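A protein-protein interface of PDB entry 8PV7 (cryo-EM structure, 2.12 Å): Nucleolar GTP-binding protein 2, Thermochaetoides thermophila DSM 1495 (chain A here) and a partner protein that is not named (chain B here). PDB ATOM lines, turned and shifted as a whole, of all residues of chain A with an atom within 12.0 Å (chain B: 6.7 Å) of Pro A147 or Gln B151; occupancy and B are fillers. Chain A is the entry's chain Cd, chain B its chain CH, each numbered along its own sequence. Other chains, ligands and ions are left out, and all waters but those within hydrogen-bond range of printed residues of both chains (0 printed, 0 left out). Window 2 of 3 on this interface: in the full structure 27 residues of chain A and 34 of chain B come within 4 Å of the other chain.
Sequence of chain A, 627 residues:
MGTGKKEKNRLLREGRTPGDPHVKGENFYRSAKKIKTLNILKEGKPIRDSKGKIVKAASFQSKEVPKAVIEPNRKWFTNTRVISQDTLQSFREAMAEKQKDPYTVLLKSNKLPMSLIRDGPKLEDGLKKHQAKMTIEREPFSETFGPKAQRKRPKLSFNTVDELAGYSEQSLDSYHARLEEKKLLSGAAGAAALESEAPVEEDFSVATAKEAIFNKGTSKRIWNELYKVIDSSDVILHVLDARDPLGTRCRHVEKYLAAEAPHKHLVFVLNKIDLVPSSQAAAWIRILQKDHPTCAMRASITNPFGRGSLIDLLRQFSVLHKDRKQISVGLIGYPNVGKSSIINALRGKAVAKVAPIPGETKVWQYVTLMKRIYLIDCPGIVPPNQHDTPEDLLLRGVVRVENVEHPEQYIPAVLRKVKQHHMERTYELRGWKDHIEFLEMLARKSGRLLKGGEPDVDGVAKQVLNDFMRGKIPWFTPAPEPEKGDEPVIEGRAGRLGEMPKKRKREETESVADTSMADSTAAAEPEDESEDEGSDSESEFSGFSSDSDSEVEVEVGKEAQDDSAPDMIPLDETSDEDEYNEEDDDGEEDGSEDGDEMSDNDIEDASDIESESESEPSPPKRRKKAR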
ATOM      1  N   PRO A 140       0.683  10.996  -0.849  1.00  0.00           N
ATOM      2  CA  PRO A 140      -0.151  11.913  -1.636  1.00  0.00           C
ATOM      3  C   PRO A 140       0.618  12.532  -2.793  1.00  0.00           C
ATOM      4  O   PRO A 140       1.849  12.493  -2.840  1.00  0.00           O
ATOM      5  CB  PRO A 140      -0.582  12.975  -0.618  1.00  0.00           C
ATOM      6  CG  PRO A 140       0.270  12.778   0.569  1.00  0.00           C
ATOM      7  CD  PRO A 140       0.735  11.368   0.572  1.00  0.00           C
ATOM      8  N   PHE A 141      -0.141  13.088  -3.744  1.00  0.00           N
ATOM      9  CA  PHE A 141       0.443  13.610  -4.976  1.00  0.00           C
ATOM     10  C   PHE A 141       1.393  14.770  -4.705  1.00  0.00           C
ATOM     11  O   PHE A 141       2.446  14.875  -5.339  1.00  0.00           O
ATOM     12  CB  PHE A 141      -0.661  14.055  -5.939  1.00  0.00           C
ATOM     13  CG  PHE A 141      -1.254  12.940  -6.750  1.00  0.00           C
ATOM     14  CD1 PHE A 141      -0.483  12.245  -7.666  1.00  0.00           C
ATOM     15  CD2 PHE A 141      -2.589  12.596  -6.609  1.00  0.00           C
ATOM     16  CE1 PHE A 141      -1.027  11.226  -8.416  1.00  0.00           C
ATOM     17  CE2 PHE A 141      -3.136  11.576  -7.355  1.00  0.00           C
ATOM     18  CZ  PHE A 141      -2.355  10.890  -8.261  1.00  0.00           C
ATOM     19  N   SER A 142       1.047  15.639  -3.755  1.00  0.00           N
ATOM     20  CA  SER A 142       1.860  16.819  -3.488  1.00  0.00           C
ATOM     21  C   SER A 142       3.175  16.485  -2.790  1.00  0.00           C
ATOM     22  O   SER A 142       4.118  17.278  -2.866  1.00  0.00           O
ATOM     23  CB  SER A 142       1.064  17.820  -2.655  1.00  0.00           C
ATOM     24  OG  SER A 142       0.634  17.231  -1.446  1.00  0.00           O
ATOM     25  N   GLU A 143       3.259  15.343  -2.119  1.00  0.00           N
ATOM     26  CA  GLU A 143       4.512  14.917  -1.513  1.00  0.00           C
ATOM     27  C   GLU A 143       5.396  14.140  -2.476  1.00  0.00           C
ATOM     28  O   GLU A 143       6.550  13.859  -2.148  1.00  0.00           O
ATOM     29  CB  GLU A 143       4.236  14.060  -0.275  1.00  0.00           C
ATOM     30  CG  GLU A 143       3.520  14.795   0.839  1.00  0.00           C
ATOM     31  CD  GLU A 143       3.256  13.916   2.047  1.00  0.00           C
ATOM     32  OE1 GLU A 143       3.705  12.752   2.049  1.00  0.00           O
ATOM     33  OE2 GLU A 143       2.580  14.385   2.986  1.00  0.00           O
ATOM     34  N   THR A 144       4.880  13.789  -3.654  1.00  0.00           N
ATOM     35  CA  THR A 144       5.647  12.974  -4.590  1.00  0.00           C
ATOM     36  C   THR A 144       6.416  13.842  -5.578  1.00  0.00           C
ATOM     37  O   THR A 144       7.644  13.747  -5.666  1.00  0.00           O
ATOM     38  CB  THR A 144       4.713  12.006  -5.317  1.00  0.00           C
ATOM     39  OG1 THR A 144       4.002  11.225  -4.354  1.00  0.00           O
ATOM     40  CG2 THR A 144       5.489  11.076  -6.217  1.00  0.00           C
ATOM     41  N   PHE A 145       5.721  14.700  -6.320  1.00  0.00           N
ATOM     42  CA  PHE A 145       6.374  15.630  -7.230  1.00  0.00           C
ATOM     43  C   PHE A 145       5.729  16.994  -7.052  1.00  0.00           C
ATOM     44  O   PHE A 145       4.530  17.095  -6.790  1.00  0.00           O
ATOM     45  CB  PHE A 145       6.269  15.162  -8.693  1.00  0.00           C
ATOM     46  CG  PHE A 145       7.258  15.815  -9.628  1.00  0.00           C
ATOM     47  CD1 PHE A 145       8.582  15.419  -9.642  1.00  0.00           C
ATOM     48  CD2 PHE A 145       6.855  16.793 -10.516  1.00  0.00           C
ATOM     49  CE1 PHE A 145       9.491  16.007 -10.498  1.00  0.00           C
ATOM     50  CE2 PHE A 145       7.756  17.375 -11.379  1.00  0.00           C
ATOM     51  CZ  PHE A 145       9.079  16.983 -11.366  1.00  0.00           C
ATOM     52  N   GLY A 146       6.530  18.044  -7.187  1.00  0.00           N
ATOM     53  CA  GLY A 146       6.040  19.392  -7.028  1.00  0.00           C
ATOM     54  C   GLY A 146       6.913  20.226  -6.113  1.00  0.00           C
ATOM     55  O   GLY A 146       7.904  19.744  -5.563  1.00  0.00           O
ATOM     56  N   PRO A 147       6.560  21.503  -5.944  1.00  0.00           N
ATOM     57  CA  PRO A 147       7.393  22.401  -5.122  1.00  0.00           C
ATOM     58  C   PRO A 147       7.472  22.028  -3.650  1.00  0.00           C
ATOM     59  O   PRO A 147       8.439  22.416  -2.988  1.00  0.00           O
ATOM     60  CB  PRO A 147       6.734  23.772  -5.319  1.00  0.00           C
ATOM     61  CG  PRO A 147       5.358  23.478  -5.802  1.00  0.00           C
ATOM     62  CD  PRO A 147       5.455  22.219  -6.600  1.00  0.00           C
ATOM     63  N   LYS A 148       6.509  21.277  -3.116  1.00  0.00           N
ATOM     64  CA  LYS A 148       6.538  20.859  -1.720  1.00  0.00           C
ATOM     65  C   LYS A 148       6.826  19.372  -1.564  1.00  0.00           C
ATOM     66  O   LYS A 148       6.598  18.815  -0.489  1.00  0.00           O
ATOM     67  CB  LYS A 148       5.221  21.206  -1.024  1.00  0.00           C
ATOM     68  CG  LYS A 148       4.805  22.656  -1.138  1.00  0.00           C
ATOM     69  CD  LYS A 148       5.903  23.599  -0.683  1.00  0.00           C
ATOM     70  CE  LYS A 148       5.545  25.039  -1.008  1.00  0.00           C
ATOM     71  NZ  LYS A 148       6.644  25.976  -0.661  1.00  0.00           N
ATOM     72  N   ALA A 149       7.318  18.722  -2.616  1.00  0.00           N
ATOM     73  CA  ALA A 149       7.523  17.282  -2.588  1.00  0.00           C
ATOM     74  C   ALA A 149       8.643  16.899  -1.630  1.00  0.00           C
ATOM     75  O   ALA A 149       9.683  17.556  -1.555  1.00  0.00           O
ATOM     76  CB  ALA A 149       7.842  16.766  -3.987  1.00  0.00           C
ATOM     77  N   GLN A 150       8.423  15.807  -0.909  1.00  0.00           N
ATOM     78  CA  GLN A 150       9.372  15.293   0.061  1.00  0.00           C
ATOM     79  C   GLN A 150       9.939  13.937  -0.321  1.00  0.00           C
ATOM     80  O   GLN A 150      10.662  13.339   0.481  1.00  0.00           O
ATOM     81  CB  GLN A 150       8.709  15.197   1.441  1.00  0.00           C
ATOM     82  CG  GLN A 150       8.172  16.516   1.948  1.00  0.00           C
ATOM     83  CD  GLN A 150       9.250  17.573   2.049  1.00  0.00           C
ATOM     84  OE1 GLN A 150      10.264  17.374   2.712  1.00  0.00           O
ATOM     85  NE2 GLN A 150       9.046  18.693   1.378  1.00  0.00           N
ATOM     86  N   ARG A 151       9.631  13.433  -1.513  1.00  0.00           N
ATOM     87  CA  ARG A 151      10.076  12.107  -1.910  1.00  0.00           C
ATOM     88  C   ARG A 151      11.564  12.114  -2.240  1.00  0.00           C
ATOM     89  O   ARG A 151      12.026  12.885  -3.081  1.00  0.00           O
ATOM     90  CB  ARG A 151       9.264  11.628  -3.112  1.00  0.00           C
ATOM     91  CG  ARG A 151       9.846  10.444  -3.856  1.00  0.00           C
ATOM     92  CD  ARG A 151       8.924  10.021  -4.986  1.00  0.00           C
ATOM     93  NE  ARG A 151       9.475   8.938  -5.793  1.00  0.00           N
ATOM     94  CZ  ARG A 151      10.061   9.104  -6.970  1.00  0.00           C
ATOM     95  NH1 ARG A 151      10.207  10.302  -7.505  1.00  0.00           N
ATOM     96  NH2 ARG A 151      10.517   8.042  -7.622  1.00  0.00           N
ATOM     97  N   LYS A 152      12.300  11.253  -1.580  1.00  0.00           N
ATOM     98  CA  LYS A 152      13.734  11.140  -1.805  1.00  0.00           C
ATOM     99  C   LYS A 152      14.150   9.768  -2.308  1.00  0.00           C
ATOM    100  O   LYS A 152      15.036   9.679  -3.151  1.00  0.00           O
ATOM    101  CB  LYS A 152      14.500  11.474  -0.514  1.00  0.00           C
ATOM    102  CG  LYS A 152      14.569  12.956  -0.212  1.00  0.00           C
ATOM    103  CD  LYS A 152      15.595  13.635  -1.089  1.00  0.00           C
ATOM    104  CE  LYS A 152      15.754  15.097  -0.731  1.00  0.00           C
ATOM    105  NZ  LYS A 152      16.731  15.759  -1.627  1.00  0.00           N
ATOM    106  N   VAL B  10      -2.076  21.669 -18.343  1.00  0.00           N
ATOM    107  CA  VAL B  10      -3.084  20.964 -17.560  1.00  0.00           C
ATOM    108  C   VAL B  10      -3.669  21.952 -16.555  1.00  0.00           C
ATOM    109  O   VAL B  10      -2.959  22.361 -15.623  1.00  0.00           O
ATOM    110  CB  VAL B  10      -2.489  19.738 -16.856  1.00  0.00           C
ATOM    111  CG1 VAL B  10      -3.509  19.097 -15.942  1.00  0.00           C
ATOM    112  CG2 VAL B  10      -1.983  18.743 -17.880  1.00  0.00           C
ATOM    113  N   TYR B  85       9.389  10.887 -11.534  1.00  0.00           N
ATOM    114  CA  TYR B  85       8.043  10.906 -10.985  1.00  0.00           C
ATOM    115  C   TYR B  85       7.707   9.467 -10.654  1.00  0.00           C
ATOM    116  O   TYR B  85       8.069   8.575 -11.413  1.00  0.00           O
ATOM    117  CB  TYR B  85       7.053  11.485 -11.998  1.00  0.00           C
ATOM    118  CG  TYR B  85       7.717  12.251 -13.121  1.00  0.00           C
ATOM    119  CD1 TYR B  85       8.084  13.583 -12.955  1.00  0.00           C
ATOM    120  CD2 TYR B  85       7.998  11.644 -14.337  1.00  0.00           C
ATOM    121  CE1 TYR B  85       8.695  14.282 -13.964  1.00  0.00           C
ATOM    122  CE2 TYR B  85       8.617  12.339 -15.356  1.00  0.00           C
ATOM    123  CZ  TYR B  85       8.962  13.661 -15.164  1.00  0.00           C
ATOM    124  OH  TYR B  85       9.576  14.374 -16.166  1.00  0.00           O
ATOM    125  N   LEU B 146      -4.531  16.749 -11.135  1.00  0.00           N
ATOM    126  CA  LEU B 146      -4.310  17.783 -12.145  1.00  0.00           C
ATOM    127  C   LEU B 146      -3.089  18.636 -11.815  1.00  0.00           C
ATOM    128  O   LEU B 146      -2.296  18.972 -12.704  1.00  0.00           O
ATOM    129  CB  LEU B 146      -5.562  18.647 -12.292  1.00  0.00           C
ATOM    130  CG  LEU B 146      -6.760  17.958 -12.952  1.00  0.00           C
ATOM    131  CD1 LEU B 146      -7.979  18.865 -13.011  1.00  0.00           C
ATOM    132  CD2 LEU B 146      -6.402  17.447 -14.325  1.00  0.00           C
ATOM    133  N   ILE B 147      -2.917  18.981 -10.536  1.00  0.00           N
ATOM    134  CA  ILE B 147      -1.736  19.722 -10.095  1.00  0.00           C
ATOM    135  C   ILE B 147      -0.471  18.907 -10.338  1.00  0.00           C
ATOM    136  O   ILE B 147       0.524  19.410 -10.890  1.00  0.00           O
ATOM    137  CB  ILE B 147      -1.883  20.099  -8.609  1.00  0.00           C
ATOM    138  CG1 ILE B 147      -3.090  21.006  -8.389  1.00  0.00           C
ATOM    139  CG2 ILE B 147      -0.615  20.734  -8.073  1.00  0.00           C
ATOM    140  CD1 ILE B 147      -3.577  20.999  -6.968  1.00  0.00           C
ATOM    141  N   TYR B 148      -0.507  17.627  -9.954  1.00  0.00           N
ATOM    142  CA  TYR B 148       0.640  16.747 -10.151  1.00  0.00           C
ATOM    143  C   TYR B 148       0.992  16.605 -11.630  1.00  0.00           C
ATOM    144  O   TYR B 148       2.170  16.661 -12.005  1.00  0.00           O
ATOM    145  CB  TYR B 148       0.339  15.387  -9.524  1.00  0.00           C
ATOM    146  CG  TYR B 148       1.246  14.259  -9.946  1.00  0.00           C
ATOM    147  CD1 TYR B 148       2.469  14.057  -9.322  1.00  0.00           C
ATOM    148  CD2 TYR B 148       0.874  13.383 -10.956  1.00  0.00           C
ATOM    149  CE1 TYR B 148       3.296  13.018  -9.697  1.00  0.00           C
ATOM    150  CE2 TYR B 148       1.694  12.348 -11.339  1.00  0.00           C
ATOM    151  CZ  TYR B 148       2.902  12.166 -10.706  1.00  0.00           C
ATOM    152  OH  TYR B 148       3.713  11.134 -11.096  1.00  0.00           O
ATOM    153  N   LEU B 149      -0.020  16.440 -12.483  1.00  0.00           N
ATOM    154  CA  LEU B 149       0.213  16.237 -13.906  1.00  0.00           C
ATOM    155  C   LEU B 149       0.713  17.495 -14.588  1.00  0.00           C
ATOM    156  O   LEU B 149       1.508  17.402 -15.520  1.00  0.00           O
ATOM    157  CB  LEU B 149      -1.055  15.745 -14.595  1.00  0.00           C
ATOM    158  CG  LEU B 149      -1.344  14.262 -14.408  1.00  0.00           C
ATOM    159  CD1 LEU B 149      -2.684  13.892 -15.026  1.00  0.00           C
ATOM    160  CD2 LEU B 149      -0.226  13.439 -14.992  1.00  0.00           C
ATOM    161  N   ASP B 150       0.279  18.674 -14.137  1.00  0.00           N
ATOM    162  CA  ASP B 150       0.826  19.907 -14.694  1.00  0.00           C
ATOM    163  C   ASP B 150       2.300  20.084 -14.335  1.00  0.00           C
ATOM    164  O   ASP B 150       3.109  20.487 -15.189  1.00  0.00           O
ATOM    165  CB  ASP B 150       0.007  21.103 -14.224  1.00  0.00           C
ATOM    166  CG  ASP B 150       0.172  22.302 -15.126  1.00  0.00           C
ATOM    167  OD1 ASP B 150       0.256  22.114 -16.355  1.00  0.00           O
ATOM    168  OD2 ASP B 150       0.238  23.432 -14.608  1.00  0.00           O
ATOM    169  N   GLN B 151       2.673  19.768 -13.087  1.00  0.00           N
ATOM    170  CA  GLN B 151       4.091  19.815 -12.717  1.00  0.00           C
ATOM    171  C   GLN B 151       4.921  18.826 -13.536  1.00  0.00           C
ATOM    172  O   GLN B 151       6.016  19.166 -14.026  1.00  0.00           O
ATOM    173  CB  GLN B 151       4.261  19.533 -11.224  1.00  0.00           C
ATOM    174  CG  GLN B 151       3.652  20.577 -10.324  1.00  0.00           C
ATOM    175  CD  GLN B 151       4.403  21.891 -10.365  1.00  0.00           C
ATOM    176  OE1 GLN B 151       5.611  21.924 -10.585  1.00  0.00           O
ATOM    177  NE2 GLN B 151       3.686  22.986 -10.164  1.00  0.00           N
ATOM    178  N   VAL B 152       4.400  17.607 -13.709  1.00  0.00           N
ATOM    179  CA  VAL B 152       5.072  16.591 -14.516  1.00  0.00           C
ATOM    180  C   VAL B 152       5.206  17.052 -15.964  1.00  0.00           C
ATOM    181  O   VAL B 152       6.235  16.821 -16.606  1.00  0.00           O
ATOM    182  CB  VAL B 152       4.324  15.246 -14.400  1.00  0.00           C
ATOM    183  CG1 VAL B 152       4.765  14.256 -15.472  1.00  0.00           C
ATOM    184  CG2 VAL B 152       4.520  14.641 -13.026  1.00  0.00           C
ATOM    185  N   ARG B 153       4.189  17.741 -16.487  1.00  0.00           N
ATOM    186  CA  ARG B 153       4.245  18.251 -17.853  1.00  0.00           C
ATOM    187  C   ARG B 153       5.357  19.279 -18.030  1.00  0.00           C
ATOM    188  O   ARG B 153       6.079  19.252 -19.031  1.00  0.00           O
ATOM    189  CB  ARG B 153       2.903  18.862 -18.245  1.00  0.00           C
ATOM    190  CG  ARG B 153       2.946  19.616 -19.551  1.00  0.00           C
ATOM    191  CD  ARG B 153       1.823  20.592 -19.699  1.00  0.00           C
ATOM    192  NE  ARG B 153       1.954  21.795 -18.886  1.00  0.00           N
ATOM    193  CZ  ARG B 153       2.527  22.916 -19.296  1.00  0.00           C
ATOM    194  NH1 ARG B 153       3.122  22.998 -20.472  1.00  0.00           N
ATOM    195  NH2 ARG B 153       2.500  23.985 -18.506  1.00  0.00           N
ATOM    196  N   GLN B 154       5.510  20.196 -17.072  1.00  0.00           N
ATOM    197  CA  GLN B 154       6.579  21.188 -17.198  1.00  0.00           C
ATOM    198  C   GLN B 154       7.964  20.541 -17.150  1.00  0.00           C
ATOM    199  O   GLN B 154       8.837  20.849 -17.981  1.00  0.00           O
ATOM    200  CB  GLN B 154       6.437  22.250 -16.116  1.00  0.00           C
ATOM    201  CG  GLN B 154       5.225  23.122 -16.310  1.00  0.00           C
ATOM    202  CD  GLN B 154       5.221  24.341 -15.423  1.00  0.00           C
ATOM    203  OE1 GLN B 154       6.227  24.685 -14.811  1.00  0.00           O
ATOM    204  NE2 GLN B 154       4.082  25.004 -15.348  1.00  0.00           N
ATOM    205  N   HIS B 155       8.167  19.603 -16.219  1.00  0.00           N
ATOM    206  CA  HIS B 155       9.463  18.932 -16.136  1.00  0.00           C
ATOM    207  C   HIS B 155       9.755  18.110 -17.396  1.00  0.00           C
ATOM    208  O   HIS B 155      10.877  18.141 -17.926  1.00  0.00           O
ATOM    209  CB  HIS B 155       9.512  18.064 -14.880  1.00  0.00           C
ATOM    210  CG  HIS B 155      10.895  17.692 -14.450  1.00  0.00           C
ATOM    211  ND1 HIS B 155      11.522  16.541 -14.868  1.00  0.00           N
ATOM    212  CD2 HIS B 155      11.769  18.318 -13.627  1.00  0.00           C
ATOM    213  CE1 HIS B 155      12.721  16.471 -14.321  1.00  0.00           C
ATOM    214  NE2 HIS B 155      12.896  17.538 -13.565  1.00  0.00           N
ATOM    215  N   LEU B 156       8.740  17.405 -17.910  1.00  0.00           N
ATOM    216  CA  LEU B 156       8.874  16.647 -19.150  1.00  0.00           C
ATOM    217  C   LEU B 156       9.166  17.545 -20.338  1.00  0.00           C
ATOM    218  O   LEU B 156       9.866  17.130 -21.266  1.00  0.00           O
ATOM    219  CB  LEU B 156       7.596  15.857 -19.422  1.00  0.00           C
ATOM    220  CG  LEU B 156       7.462  14.498 -18.760  1.00  0.00           C
ATOM    221  CD1 LEU B 156       6.064  13.966 -18.979  1.00  0.00           C
ATOM    222  CD2 LEU B 156       8.494  13.561 -19.319  1.00  0.00           C
ATOM    223  N   ARG B 158      10.934  20.224 -20.165  1.00  0.00           N
ATOM    224  CA  ARG B 158      12.328  20.642 -20.063  1.00  0.00           C
ATOM    225  C   ARG B 158      13.327  19.485 -20.040  1.00  0.00           C
ATOM    226  O   ARG B 158      14.522  19.740 -19.890  1.00  0.00           O
ATOM    227  CB  ARG B 158      12.518  21.529 -18.830  1.00  0.00           C
ATOM    228  CG  ARG B 158      11.622  22.760 -18.853  1.00  0.00           C
ATOM    229  CD  ARG B 158      12.001  23.792 -17.811  1.00  0.00           C
ATOM    230  NE  ARG B 158      12.024  23.228 -16.469  1.00  0.00           N
ATOM    231  CZ  ARG B 158      10.973  23.150 -15.669  1.00  0.00           C
ATOM    232  NH1 ARG B 158       9.781  23.573 -16.049  1.00  0.00           N
ATOM    233  NH2 ARG B 158      11.124  22.626 -14.457  1.00  0.00           N
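The side-chain hydroxyl of Tyr B85 sits at hydrogen-bond distance from a ring nitrogen (ND1) of His B155 (3.2 Å).
Tyr B148 touches Phe A141 (CG to CD1, 3.5 Å). CD1 of Tyr B85 touches CE1 of Phe A145, at 3.7 Å. Tyr B148 touches Phe A145. CE2 of Phe A145 touches O of Gln B151, at 3.6 Å. CG of His B155 touches CZ of Phe A145 (3.6 Å). CD of Gln B151 touches CD of Pro A147 (3.9 Å).
Pro A140 touches none of the printed residues of chain B. Printed residues of chain B within 4 Å of Phe A141: Tyr B148. Pro A147 touches just one residue of chain B: Gln B151. No residue of chain A comes within 4 Å of Val B10. Printed residues of chain A within 4 Å of Tyr B85: Phe A145 (3.7 Å). Of the printed residues of chain A, Tyr B148 touches Phe A141 (3.5 Å) and Phe A145 (3.8 Å). No residue of chain A comes within 4 Å of Asp B150. Of chain A, only Phe A145 and Pro A147 come within 4 Å of Gln B151. His B155 touches just one residue of chain A: Phe A145. Arg B158 touches none of the printed residues of chain A. The nearest residue of chain B that does not touch Pro A147 is Ile B147 (6.4 Å). The nearest printed residue of chain A that does not touch Tyr B148 is Thr A144 (4.5 Å).
Printed residues of chain A that touch a printed residue of chain B: Phe A141, Phe A145 and Pro A147. Hydrophobic or aromatic side chains of chain A within 4 Å of the printed part of chain B: Phe A141, Phe A145 and Pro A147. Along chain A the printed residues that touch a printed residue of chain B span positions 141 to 147. Of the 14 printed residues of chain B, 4 touch a printed residue of chain A. Printed residues of chain B that touch a printed residue of chain A: Tyr B85, Tyr B148, Gln B151 and His B155. Hydrophobic or aromatic side chains of chain B within 4 Å of the printed part of chain A: Tyr B85, Tyr B148 and His B155. Among the printed residues, 6 pairs touch across the chains.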
